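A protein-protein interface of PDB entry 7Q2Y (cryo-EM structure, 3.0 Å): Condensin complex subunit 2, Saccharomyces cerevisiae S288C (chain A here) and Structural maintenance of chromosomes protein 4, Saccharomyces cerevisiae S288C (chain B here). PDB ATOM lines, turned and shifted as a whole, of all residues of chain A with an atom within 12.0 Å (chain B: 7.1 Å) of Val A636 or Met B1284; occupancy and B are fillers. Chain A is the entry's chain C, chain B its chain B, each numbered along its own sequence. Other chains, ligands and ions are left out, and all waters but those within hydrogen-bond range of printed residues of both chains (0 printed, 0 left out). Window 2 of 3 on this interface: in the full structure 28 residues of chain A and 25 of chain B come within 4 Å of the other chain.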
ATOM      1  N   LYS A 635      19.026 -23.194 -14.956  1.00  0.00           N
ATOM      2  CA  LYS A 635      19.752 -22.327 -14.036  1.00  0.00           C
ATOM      3  C   LYS A 635      19.792 -22.927 -12.634  1.00  0.00           C
ATOM      4  O   LYS A 635      20.627 -22.551 -11.811  1.00  0.00           O
ATOM      5  CB  LYS A 635      19.116 -20.936 -13.996  1.00  0.00           C
ATOM      6  N   VAL A 636      18.882 -23.860 -12.369  1.00  0.00           N
ATOM      7  CA  VAL A 636      18.792 -24.533 -11.078  1.00  0.00           C
ATOM      8  C   VAL A 636      19.132 -26.002 -11.282  1.00  0.00           C
ATOM      9  O   VAL A 636      18.494 -26.690 -12.088  1.00  0.00           O
ATOM     10  CB  VAL A 636      17.397 -24.368 -10.456  1.00  0.00           C
ATOM     11  CG1 VAL A 636      17.290 -25.178  -9.172  1.00  0.00           C
ATOM     12  CG2 VAL A 636      17.104 -22.900 -10.192  1.00  0.00           C
ATOM     13  N   THR A 637      20.138 -26.482 -10.556  1.00  0.00           N
ATOM     14  CA  THR A 637      20.547 -27.875 -10.673  1.00  0.00           C
ATOM     15  C   THR A 637      19.536 -28.792  -9.994  1.00  0.00           C
ATOM     16  O   THR A 637      18.968 -28.456  -8.953  1.00  0.00           O
ATOM     17  CB  THR A 637      21.932 -28.077 -10.060  1.00  0.00           C
ATOM     18  OG1 THR A 637      21.893 -27.747  -8.667  1.00  0.00           O
ATOM     19  CG2 THR A 637      22.955 -27.192 -10.756  1.00  0.00           C
ATOM     20  N   TYR A 638      19.314 -29.959 -10.596  1.00  0.00           N
ATOM     21  CA  TYR A 638      18.397 -30.944 -10.042  1.00  0.00           C
ATOM     22  C   TYR A 638      18.763 -32.317 -10.585  1.00  0.00           C
ATOM     23  O   TYR A 638      19.495 -32.442 -11.571  1.00  0.00           O
ATOM     24  CB  TYR A 638      16.937 -30.601 -10.362  1.00  0.00           C
ATOM     25  CG  TYR A 638      16.623 -30.504 -11.839  1.00  0.00           C
ATOM     26  CD1 TYR A 638      16.251 -31.626 -12.568  1.00  0.00           C
ATOM     27  CD2 TYR A 638      16.692 -29.286 -12.503  1.00  0.00           C
ATOM     28  CE1 TYR A 638      15.961 -31.538 -13.916  1.00  0.00           C
ATOM     29  CE2 TYR A 638      16.404 -29.190 -13.851  1.00  0.00           C
ATOM     30  CZ  TYR A 638      16.039 -30.317 -14.552  1.00  0.00           C
ATOM     31  OH  TYR A 638      15.752 -30.226 -15.895  1.00  0.00           O
ATOM     32  N   SER A 639      18.244 -33.348  -9.923  1.00  0.00           N
ATOM     33  CA  SER A 639      18.491 -34.729 -10.316  1.00  0.00           C
ATOM     34  C   SER A 639      17.504 -35.124 -11.408  1.00  0.00           C
ATOM     35  O   SER A 639      16.286 -35.087 -11.194  1.00  0.00           O
ATOM     36  CB  SER A 639      18.370 -35.664  -9.114  1.00  0.00           C
ATOM     37  OG  SER A 639      19.480 -35.522  -8.245  1.00  0.00           O
ATOM     38  N   ARG A 640      18.029 -35.502 -12.574  1.00  0.00           N
ATOM     39  CA  ARG A 640      17.173 -35.867 -13.696  1.00  0.00           C
ATOM     40  C   ARG A 640      16.572 -37.258 -13.540  1.00  0.00           C
ATOM     41  O   ARG A 640      15.462 -37.505 -14.023  1.00  0.00           O
ATOM     42  CB  ARG A 640      17.957 -35.782 -15.007  1.00  0.00           C
ATOM     43  CG  ARG A 640      17.992 -34.391 -15.627  1.00  0.00           C
ATOM     44  CD  ARG A 640      19.051 -33.516 -14.975  1.00  0.00           C
ATOM     45  NE  ARG A 640      19.078 -32.174 -15.546  1.00  0.00           N
ATOM     46  CZ  ARG A 640      19.814 -31.817 -16.589  1.00  0.00           C
ATOM     47  NH1 ARG A 640      20.604 -32.682 -17.206  1.00  0.00           N
ATOM     48  NH2 ARG A 640      19.759 -30.562 -17.024  1.00  0.00           N
ATOM     49  N   VAL A 641      17.277 -38.171 -12.876  1.00  0.00           N
ATOM     50  CA  VAL A 641      16.834 -39.552 -12.739  1.00  0.00           C
ATOM     51  C   VAL A 641      16.746 -39.905 -11.260  1.00  0.00           C
ATOM     52  O   VAL A 641      17.572 -39.481 -10.444  1.00  0.00           O
ATOM     53  CB  VAL A 641      17.768 -40.527 -13.494  1.00  0.00           C
ATOM     54  CG1 VAL A 641      19.164 -40.535 -12.883  1.00  0.00           C
ATOM     55  CG2 VAL A 641      17.176 -41.930 -13.520  1.00  0.00           C
ATOM     56  N   LEU B1278       8.895 -12.299  -5.628  1.00  0.00           N
ATOM     57  CA  LEU B1278       8.150 -13.550  -5.719  1.00  0.00           C
ATOM     58  C   LEU B1278       7.952 -13.975  -7.166  1.00  0.00           C
ATOM     59  O   LEU B1278       8.024 -15.168  -7.480  1.00  0.00           O
ATOM     60  CB  LEU B1278       6.803 -13.411  -5.010  1.00  0.00           C
ATOM     61  CG  LEU B1278       5.753 -14.476  -5.330  1.00  0.00           C
ATOM     62  CD1 LEU B1278       6.206 -15.848  -4.856  1.00  0.00           C
ATOM     63  CD2 LEU B1278       4.418 -14.113  -4.712  1.00  0.00           C
ATOM     64  N   LYS B1279       7.689 -13.020  -8.062  1.00  0.00           N
ATOM     65  CA  LYS B1279       7.574 -13.368  -9.475  1.00  0.00           C
ATOM     66  C   LYS B1279       8.875 -13.965  -9.995  1.00  0.00           C
ATOM     67  O   LYS B1279       8.873 -15.032 -10.626  1.00  0.00           O
ATOM     68  CB  LYS B1279       7.182 -12.136 -10.289  1.00  0.00           C
ATOM     69  CG  LYS B1279       6.899 -12.424 -11.753  1.00  0.00           C
ATOM     70  CD  LYS B1279       6.510 -11.158 -12.496  1.00  0.00           C
ATOM     71  CE  LYS B1279       5.129 -10.678 -12.083  1.00  0.00           C
ATOM     72  NZ  LYS B1279       4.058 -11.619 -12.513  1.00  0.00           N
ATOM     73  N   GLU B1280      10.004 -13.309  -9.704  1.00  0.00           N
ATOM     74  CA  GLU B1280      11.294 -13.847 -10.128  1.00  0.00           C
ATOM     75  C   GLU B1280      11.570 -15.198  -9.476  1.00  0.00           C
ATOM     76  O   GLU B1280      12.105 -16.110 -10.120  1.00  0.00           O
ATOM     77  CB  GLU B1280      12.411 -12.852  -9.802  1.00  0.00           C
ATOM     78  CG  GLU B1280      13.784 -13.104 -10.463  1.00  0.00           C
ATOM     79  CD  GLU B1280      13.766 -13.346 -11.978  1.00  0.00           C
ATOM     80  OE1 GLU B1280      12.697 -13.294 -12.623  1.00  0.00           O
ATOM     81  OE2 GLU B1280      14.856 -13.596 -12.534  1.00  0.00           O
ATOM     82  N   MET B1281      11.204 -15.345  -8.201  1.00  0.00           N
ATOM     83  CA  MET B1281      11.469 -16.577  -7.471  1.00  0.00           C
ATOM     84  C   MET B1281      10.693 -17.746  -8.060  1.00  0.00           C
ATOM     85  O   MET B1281      11.242 -18.837  -8.235  1.00  0.00           O
ATOM     86  CB  MET B1281      11.103 -16.386  -6.001  1.00  0.00           C
ATOM     87  CG  MET B1281      11.452 -17.554  -5.111  1.00  0.00           C
ATOM     88  SD  MET B1281      13.237 -17.761  -5.101  1.00  0.00           S
ATOM     89  CE  MET B1281      13.683 -16.333  -4.119  1.00  0.00           C
ATOM     90  N   TYR B1282       9.410 -17.535  -8.361  1.00  0.00           N
ATOM     91  CA  TYR B1282       8.610 -18.592  -8.969  1.00  0.00           C
ATOM     92  C   TYR B1282       9.110 -18.916 -10.368  1.00  0.00           C
ATOM     93  O   TYR B1282       9.160 -20.088 -10.762  1.00  0.00           O
ATOM     94  CB  TYR B1282       7.137 -18.188  -9.002  1.00  0.00           C
ATOM     95  CG  TYR B1282       6.190 -19.357  -9.146  1.00  0.00           C
ATOM     96  CD1 TYR B1282       5.984 -20.241  -8.096  1.00  0.00           C
ATOM     97  CD2 TYR B1282       5.509 -19.583 -10.334  1.00  0.00           C
ATOM     98  CE1 TYR B1282       5.123 -21.312  -8.220  1.00  0.00           C
ATOM     99  CE2 TYR B1282       4.645 -20.654 -10.470  1.00  0.00           C
ATOM    100  CZ  TYR B1282       4.456 -21.515  -9.410  1.00  0.00           C
ATOM    101  OH  TYR B1282       3.599 -22.583  -9.539  1.00  0.00           O
ATOM    102  N   GLN B1283       9.504 -17.889 -11.132  1.00  0.00           N
ATOM    103  CA  GLN B1283      10.069 -18.133 -12.454  1.00  0.00           C
ATOM    104  C   GLN B1283      11.322 -18.996 -12.368  1.00  0.00           C
ATOM    105  O   GLN B1283      11.526 -19.894 -13.193  1.00  0.00           O
ATOM    106  CB  GLN B1283      10.383 -16.805 -13.142  1.00  0.00           C
ATOM    107  CG  GLN B1283      10.197 -16.813 -14.649  1.00  0.00           C
ATOM    108  CD  GLN B1283      10.585 -15.494 -15.288  1.00  0.00           C
ATOM    109  OE1 GLN B1283      10.501 -14.438 -14.658  1.00  0.00           O
ATOM    110  NE2 GLN B1283      11.025 -15.547 -16.539  1.00  0.00           N
ATOM    111  N   MET B1284      12.173 -18.740 -11.373  1.00  0.00           N
ATOM    112  CA  MET B1284      13.420 -19.488 -11.259  1.00  0.00           C
ATOM    113  C   MET B1284      13.189 -20.891 -10.705  1.00  0.00           C
ATOM    114  O   MET B1284      13.866 -21.842 -11.112  1.00  0.00           O
ATOM    115  CB  MET B1284      14.412 -18.717 -10.390  1.00  0.00           C
ATOM    116  CG  MET B1284      15.769 -19.384 -10.248  1.00  0.00           C
ATOM    117  SD  MET B1284      16.902 -18.416  -9.236  1.00  0.00           S
ATOM    118  CE  MET B1284      16.186 -18.654  -7.615  1.00  0.00           C
ATOM    119  N   ILE B1285      12.237 -21.046  -9.783  1.00  0.00           N
ATOM    120  CA  ILE B1285      12.081 -22.328  -9.102  1.00  0.00           C
ATOM    121  C   ILE B1285      11.208 -23.289  -9.904  1.00  0.00           C
ATOM    122  O   ILE B1285      11.355 -24.511  -9.779  1.00  0.00           O
ATOM    123  CB  ILE B1285      11.528 -22.115  -7.681  1.00  0.00           C
ATOM    124  CG1 ILE B1285      11.797 -23.345  -6.812  1.00  0.00           C
ATOM    125  CG2 ILE B1285      10.038 -21.804  -7.712  1.00  0.00           C
ATOM    126  CD1 ILE B1285      11.540 -23.117  -5.339  1.00  0.00           C
ATOM    127  N   THR B1286      10.299 -22.779 -10.734  1.00  0.00           N
ATOM    128  CA  THR B1286       9.432 -23.631 -11.534  1.00  0.00           C
ATOM    129  C   THR B1286       9.853 -23.707 -12.994  1.00  0.00           C
ATOM    130  O   THR B1286       9.216 -24.428 -13.768  1.00  0.00           O
ATOM    131  CB  THR B1286       7.982 -23.147 -11.441  1.00  0.00           C
ATOM    132  OG1 THR B1286       7.906 -21.776 -11.851  1.00  0.00           O
ATOM    133  CG2 THR B1286       7.469 -23.275 -10.017  1.00  0.00           C
ATOM    134  N   MET B1287      10.913 -22.993 -13.382  1.00  0.00           N
ATOM    135  CA  MET B1287      11.392 -22.964 -14.763  1.00  0.00           C
ATOM    136  C   MET B1287      10.265 -22.586 -15.722  1.00  0.00           C
ATOM    137  O   MET B1287      10.077 -23.191 -16.780  1.00  0.00           O
ATOM    138  CB  MET B1287      12.027 -24.302 -15.149  1.00  0.00           C
ATOM    139  CG  MET B1287      13.307 -24.611 -14.391  1.00  0.00           C
ATOM    140  SD  MET B1287      14.072 -26.160 -14.903  1.00  0.00           S
ATOM    141  CE  MET B1287      12.963 -27.343 -14.147  1.00  0.00           C
ATOM    142  N   GLY B1288       9.507 -21.568 -15.335  1.00  0.00           N
ATOM    143  CA  GLY B1288       8.335 -21.141 -16.079  1.00  0.00           C
ATOM    144  C   GLY B1288       7.195 -20.867 -15.120  1.00  0.00           C
ATOM    145  O   GLY B1288       7.217 -21.271 -13.956  1.00  0.00           O
ATOM    146  N   GLY B1289       6.185 -20.165 -15.614  1.00  0.00           N
ATOM    147  CA  GLY B1289       5.034 -19.797 -14.814  1.00  0.00           C
ATOM    148  C   GLY B1289       5.212 -18.426 -14.182  1.00  0.00           C
ATOM    149  O   GLY B1289       6.273 -17.804 -14.251  1.00  0.00           O
ATOM    150  N   LYS B1341      14.501 -13.462   0.989  1.00  0.00           N
ATOM    151  CA  LYS B1341      15.394 -12.598   0.223  1.00  0.00           C
ATOM    152  C   LYS B1341      15.115 -11.127   0.509  1.00  0.00           C
ATOM    153  O   LYS B1341      16.047 -10.318   0.589  1.00  0.00           O
ATOM    154  CB  LYS B1341      15.259 -12.893  -1.270  1.00  0.00           C
ATOM    155  CG  LYS B1341      16.251 -12.143  -2.141  1.00  0.00           C
ATOM    156  CD  LYS B1341      16.067 -12.486  -3.610  1.00  0.00           C
ATOM    157  CE  LYS B1341      16.529 -13.903  -3.906  1.00  0.00           C
ATOM    158  NZ  LYS B1341      18.001 -14.052  -3.742  1.00  0.00           N
ATOM    159  N   ARG B1360      12.412 -34.402  -8.654  1.00  0.00           N
ATOM    160  CA  ARG B1360      12.975 -33.206  -9.272  1.00  0.00           C
ATOM    161  C   ARG B1360      12.696 -31.965  -8.432  1.00  0.00           C
ATOM    162  O   ARG B1360      13.584 -31.126  -8.233  1.00  0.00           O
ATOM    163  CB  ARG B1360      12.419 -33.036 -10.685  1.00  0.00           C
ATOM    164  CG  ARG B1360      12.827 -34.140 -11.646  1.00  0.00           C
ATOM    165  CD  ARG B1360      12.228 -33.932 -13.027  1.00  0.00           C
ATOM    166  NE  ARG B1360      12.763 -32.748 -13.687  1.00  0.00           N
ATOM    167  CZ  ARG B1360      12.076 -31.636 -13.906  1.00  0.00           C
ATOM    168  NH1 ARG B1360      10.815 -31.516 -13.522  1.00  0.00           N
ATOM    169  NH2 ARG B1360      12.667 -30.619 -14.527  1.00  0.00           N
ATOM    170  N   SER B1363      14.701 -32.035  -5.229  1.00  0.00           N
ATOM    171  CA  SER B1363      16.089 -31.741  -5.574  1.00  0.00           C
ATOM    172  C   SER B1363      16.295 -30.249  -5.808  1.00  0.00           C
ATOM    173  O   SER B1363      17.297 -29.676  -5.363  1.00  0.00           O
ATOM    174  CB  SER B1363      16.503 -32.537  -6.811  1.00  0.00           C
ATOM    175  OG  SER B1363      16.353 -33.929  -6.599  1.00  0.00           O
ATOM    176  N   ILE B1364      15.356 -29.605  -6.505  1.00  0.00           N
ATOM    177  CA  ILE B1364      15.454 -28.168  -6.748  1.00  0.00           C
ATOM    178  C   ILE B1364      15.422 -27.401  -5.432  1.00  0.00           C
ATOM    179  O   ILE B1364      16.217 -26.477  -5.213  1.00  0.00           O
ATOM    180  CB  ILE B1364      14.329 -27.712  -7.697  1.00  0.00           C
ATOM    181  CG1 ILE B1364      14.663 -28.078  -9.143  1.00  0.00           C
ATOM    182  CG2 ILE B1364      14.086 -26.215  -7.569  1.00  0.00           C
ATOM    183  CD1 ILE B1364      13.452 -28.168 -10.044  1.00  0.00           C
ATOM    184  N   VAL B1365      14.505 -27.773  -4.537  1.00  0.00           N
ATOM    185  CA  VAL B1365      14.401 -27.095  -3.246  1.00  0.00           C
ATOM    186  C   VAL B1365      15.676 -27.291  -2.433  1.00  0.00           C
ATOM    187  O   VAL B1365      16.188 -26.350  -1.810  1.00  0.00           O
ATOM    188  CB  VAL B1365      13.156 -27.589  -2.485  1.00  0.00           C
ATOM    189  CG1 VAL B1365      13.134 -27.027  -1.075  1.00  0.00           C
ATOM    190  CG2 VAL B1365      11.894 -27.199  -3.233  1.00  0.00           C
ATOM    191  N   ASN B1367      18.727 -27.915  -3.553  1.00  0.00           N
ATOM    192  CA  ASN B1367      19.809 -27.134  -4.144  1.00  0.00           C
ATOM    193  C   ASN B1367      19.663 -25.651  -3.821  1.00  0.00           C
ATOM    194  O   ASN B1367      20.652 -24.976  -3.501  1.00  0.00           O
ATOM    195  CB  ASN B1367      19.852 -27.355  -5.655  1.00  0.00           C
ATOM    196  CG  ASN B1367      20.568 -28.635  -6.035  1.00  0.00           C
ATOM    197  OD1 ASN B1367      19.949 -29.594  -6.494  1.00  0.00           O
ATOM    198  ND2 ASN B1367      21.882 -28.658  -5.841  1.00  0.00           N
ATOM    199  N   TYR B1368      18.438 -25.125  -3.898  1.00  0.00           N
ATOM    200  CA  TYR B1368      18.223 -23.733  -3.525  1.00  0.00           C
ATOM    201  C   TYR B1368      18.654 -23.479  -2.089  1.00  0.00           C
ATOM    202  O   TYR B1368      19.367 -22.513  -1.805  1.00  0.00           O
ATOM    203  CB  TYR B1368      16.758 -23.339  -3.720  1.00  0.00           C
ATOM    204  CG  TYR B1368      16.524 -21.865  -3.477  1.00  0.00           C
ATOM    205  CD1 TYR B1368      16.299 -21.388  -2.191  1.00  0.00           C
ATOM    206  CD2 TYR B1368      16.571 -20.949  -4.515  1.00  0.00           C
ATOM    207  CE1 TYR B1368      16.103 -20.049  -1.950  1.00  0.00           C
ATOM    208  CE2 TYR B1368      16.375 -19.600  -4.281  1.00  0.00           C
ATOM    209  CZ  TYR B1368      16.142 -19.160  -2.995  1.00  0.00           C
ATOM    210  OH  TYR B1368      15.949 -17.825  -2.740  1.00  0.00           O
ATOM    211  N   ARG B1372      21.785 -21.223  -2.665  1.00  0.00           N
ATOM    212  CA  ARG B1372      21.208 -19.885  -2.752  1.00  0.00           C
ATOM    213  C   ARG B1372      20.907 -19.269  -1.390  1.00  0.00           C
ATOM    214  O   ARG B1372      20.631 -18.067  -1.321  1.00  0.00           O
ATOM    215  CB  ARG B1372      19.935 -19.918  -3.599  1.00  0.00           C
ATOM    216  CG  ARG B1372      20.169 -20.352  -5.034  1.00  0.00           C
ATOM    217  CD  ARG B1372      20.962 -19.297  -5.788  1.00  0.00           C
ATOM    218  NE  ARG B1372      21.151 -19.640  -7.191  1.00  0.00           N
ATOM    219  CZ  ARG B1372      21.867 -18.921  -8.046  1.00  0.00           C
ATOM    220  NH1 ARG B1372      22.474 -17.807  -7.673  1.00  0.00           N
ATOM    221  NH2 ARG B1372      21.975 -19.332  -9.306  1.00  0.00           N
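The side-chain amide oxygen (OD1) of Asn B1367 sits close to the backbone carbonyl oxygen (O) of Thr A637 (2.9 Å).
NH2 of Arg B1360 sits close to OH of Tyr A638 (3.4 Å).
The side-chain amide oxygen (OD1) of Asn B1367 sits close to the backbone carbonyl oxygen (O) of Ser B1363, at 2.9 Å.
Among the printed residues, pairs that only touch across the chains: Val A636 with Met B1284, Val A636 with Ile B1364, Tyr A638 with Met B1287, Tyr A638 with Ile B1364, Ser A639 with Arg B1360 and Ser A639 with Ser B1363.
Of the printed residues of chain B, Val A636 touches Met B1284 and Ile B1364.
Glu B1280 touches none of the printed residues of chain A.
No residue of chain A comes within 4 Å of Met B1281.
No residue of chain A comes within 4 Å of Gln B1283.
No residue of chain A comes within 4 Å of Ile B1285.
No residue of chain A comes within 4 Å of Thr B1286.
Printed residues of chain A within 4 Å of Met B1287: Tyr A638.
No residue of chain A comes within 4 Å of Gly B1288.
Of chain A, only Val A636 (3.7 Å) and Tyr A638 (3.6 Å) come within 4 Å of Ile B1364.
Of chain A, only Thr A637 comes within 4 Å of Asn B1367.
No residue of chain A comes within 4 Å of Tyr B1368.
No residue of chain A comes within 4 Å of Arg B1372.
Printed residues of chain B within 4 Å of Tyr A638: Met B1287 (3.9 Å), Arg B1360 (3.4 Å) and Ile B1364 (3.6 Å).
Of the printed residues of chain B, Ser A639 touches Arg B1360 (3.6 Å) and Ser B1363 (3.7 Å).
Of the printed residues of chain A, Ser B1363 touches Ser A639 (3.7 Å).
Printed residues of chain A within 4 Å of Arg B1360: Tyr A638 (3.4 Å) and Ser A639 (3.6 Å).
The nearest residue of chain B that does not touch Val A636 is Asn B1367 (4.9 Å).
The nearest printed residue of chain B that does not touch Ser A639 is Asn B1367 (5.4 Å).
Of the 7 printed residues of chain A, 4 touch a printed residue of chain B.
Hydrophobic or aromatic side chains of chain A within 4 Å of the printed part of chain B: Val A636 and Tyr A638.
Of the 20 printed residues of chain B, 6 touch a printed residue of chain A.
Printed residues of chain B that touch a printed residue of chain A: Met B1284, Met B1287, Arg B1360, Ser B1363, Ile B1364 and Asn B1367.
Hydrophobic or aromatic side chains of chain B within 4 Å of the printed part of chain A: Met B1284, Met B1287 and Ile B1364.
Along chain B the printed residues that touch a printed residue of chain A span positions 1284 to 1367.
Among the printed residues, 8 pairs touch across the chains.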
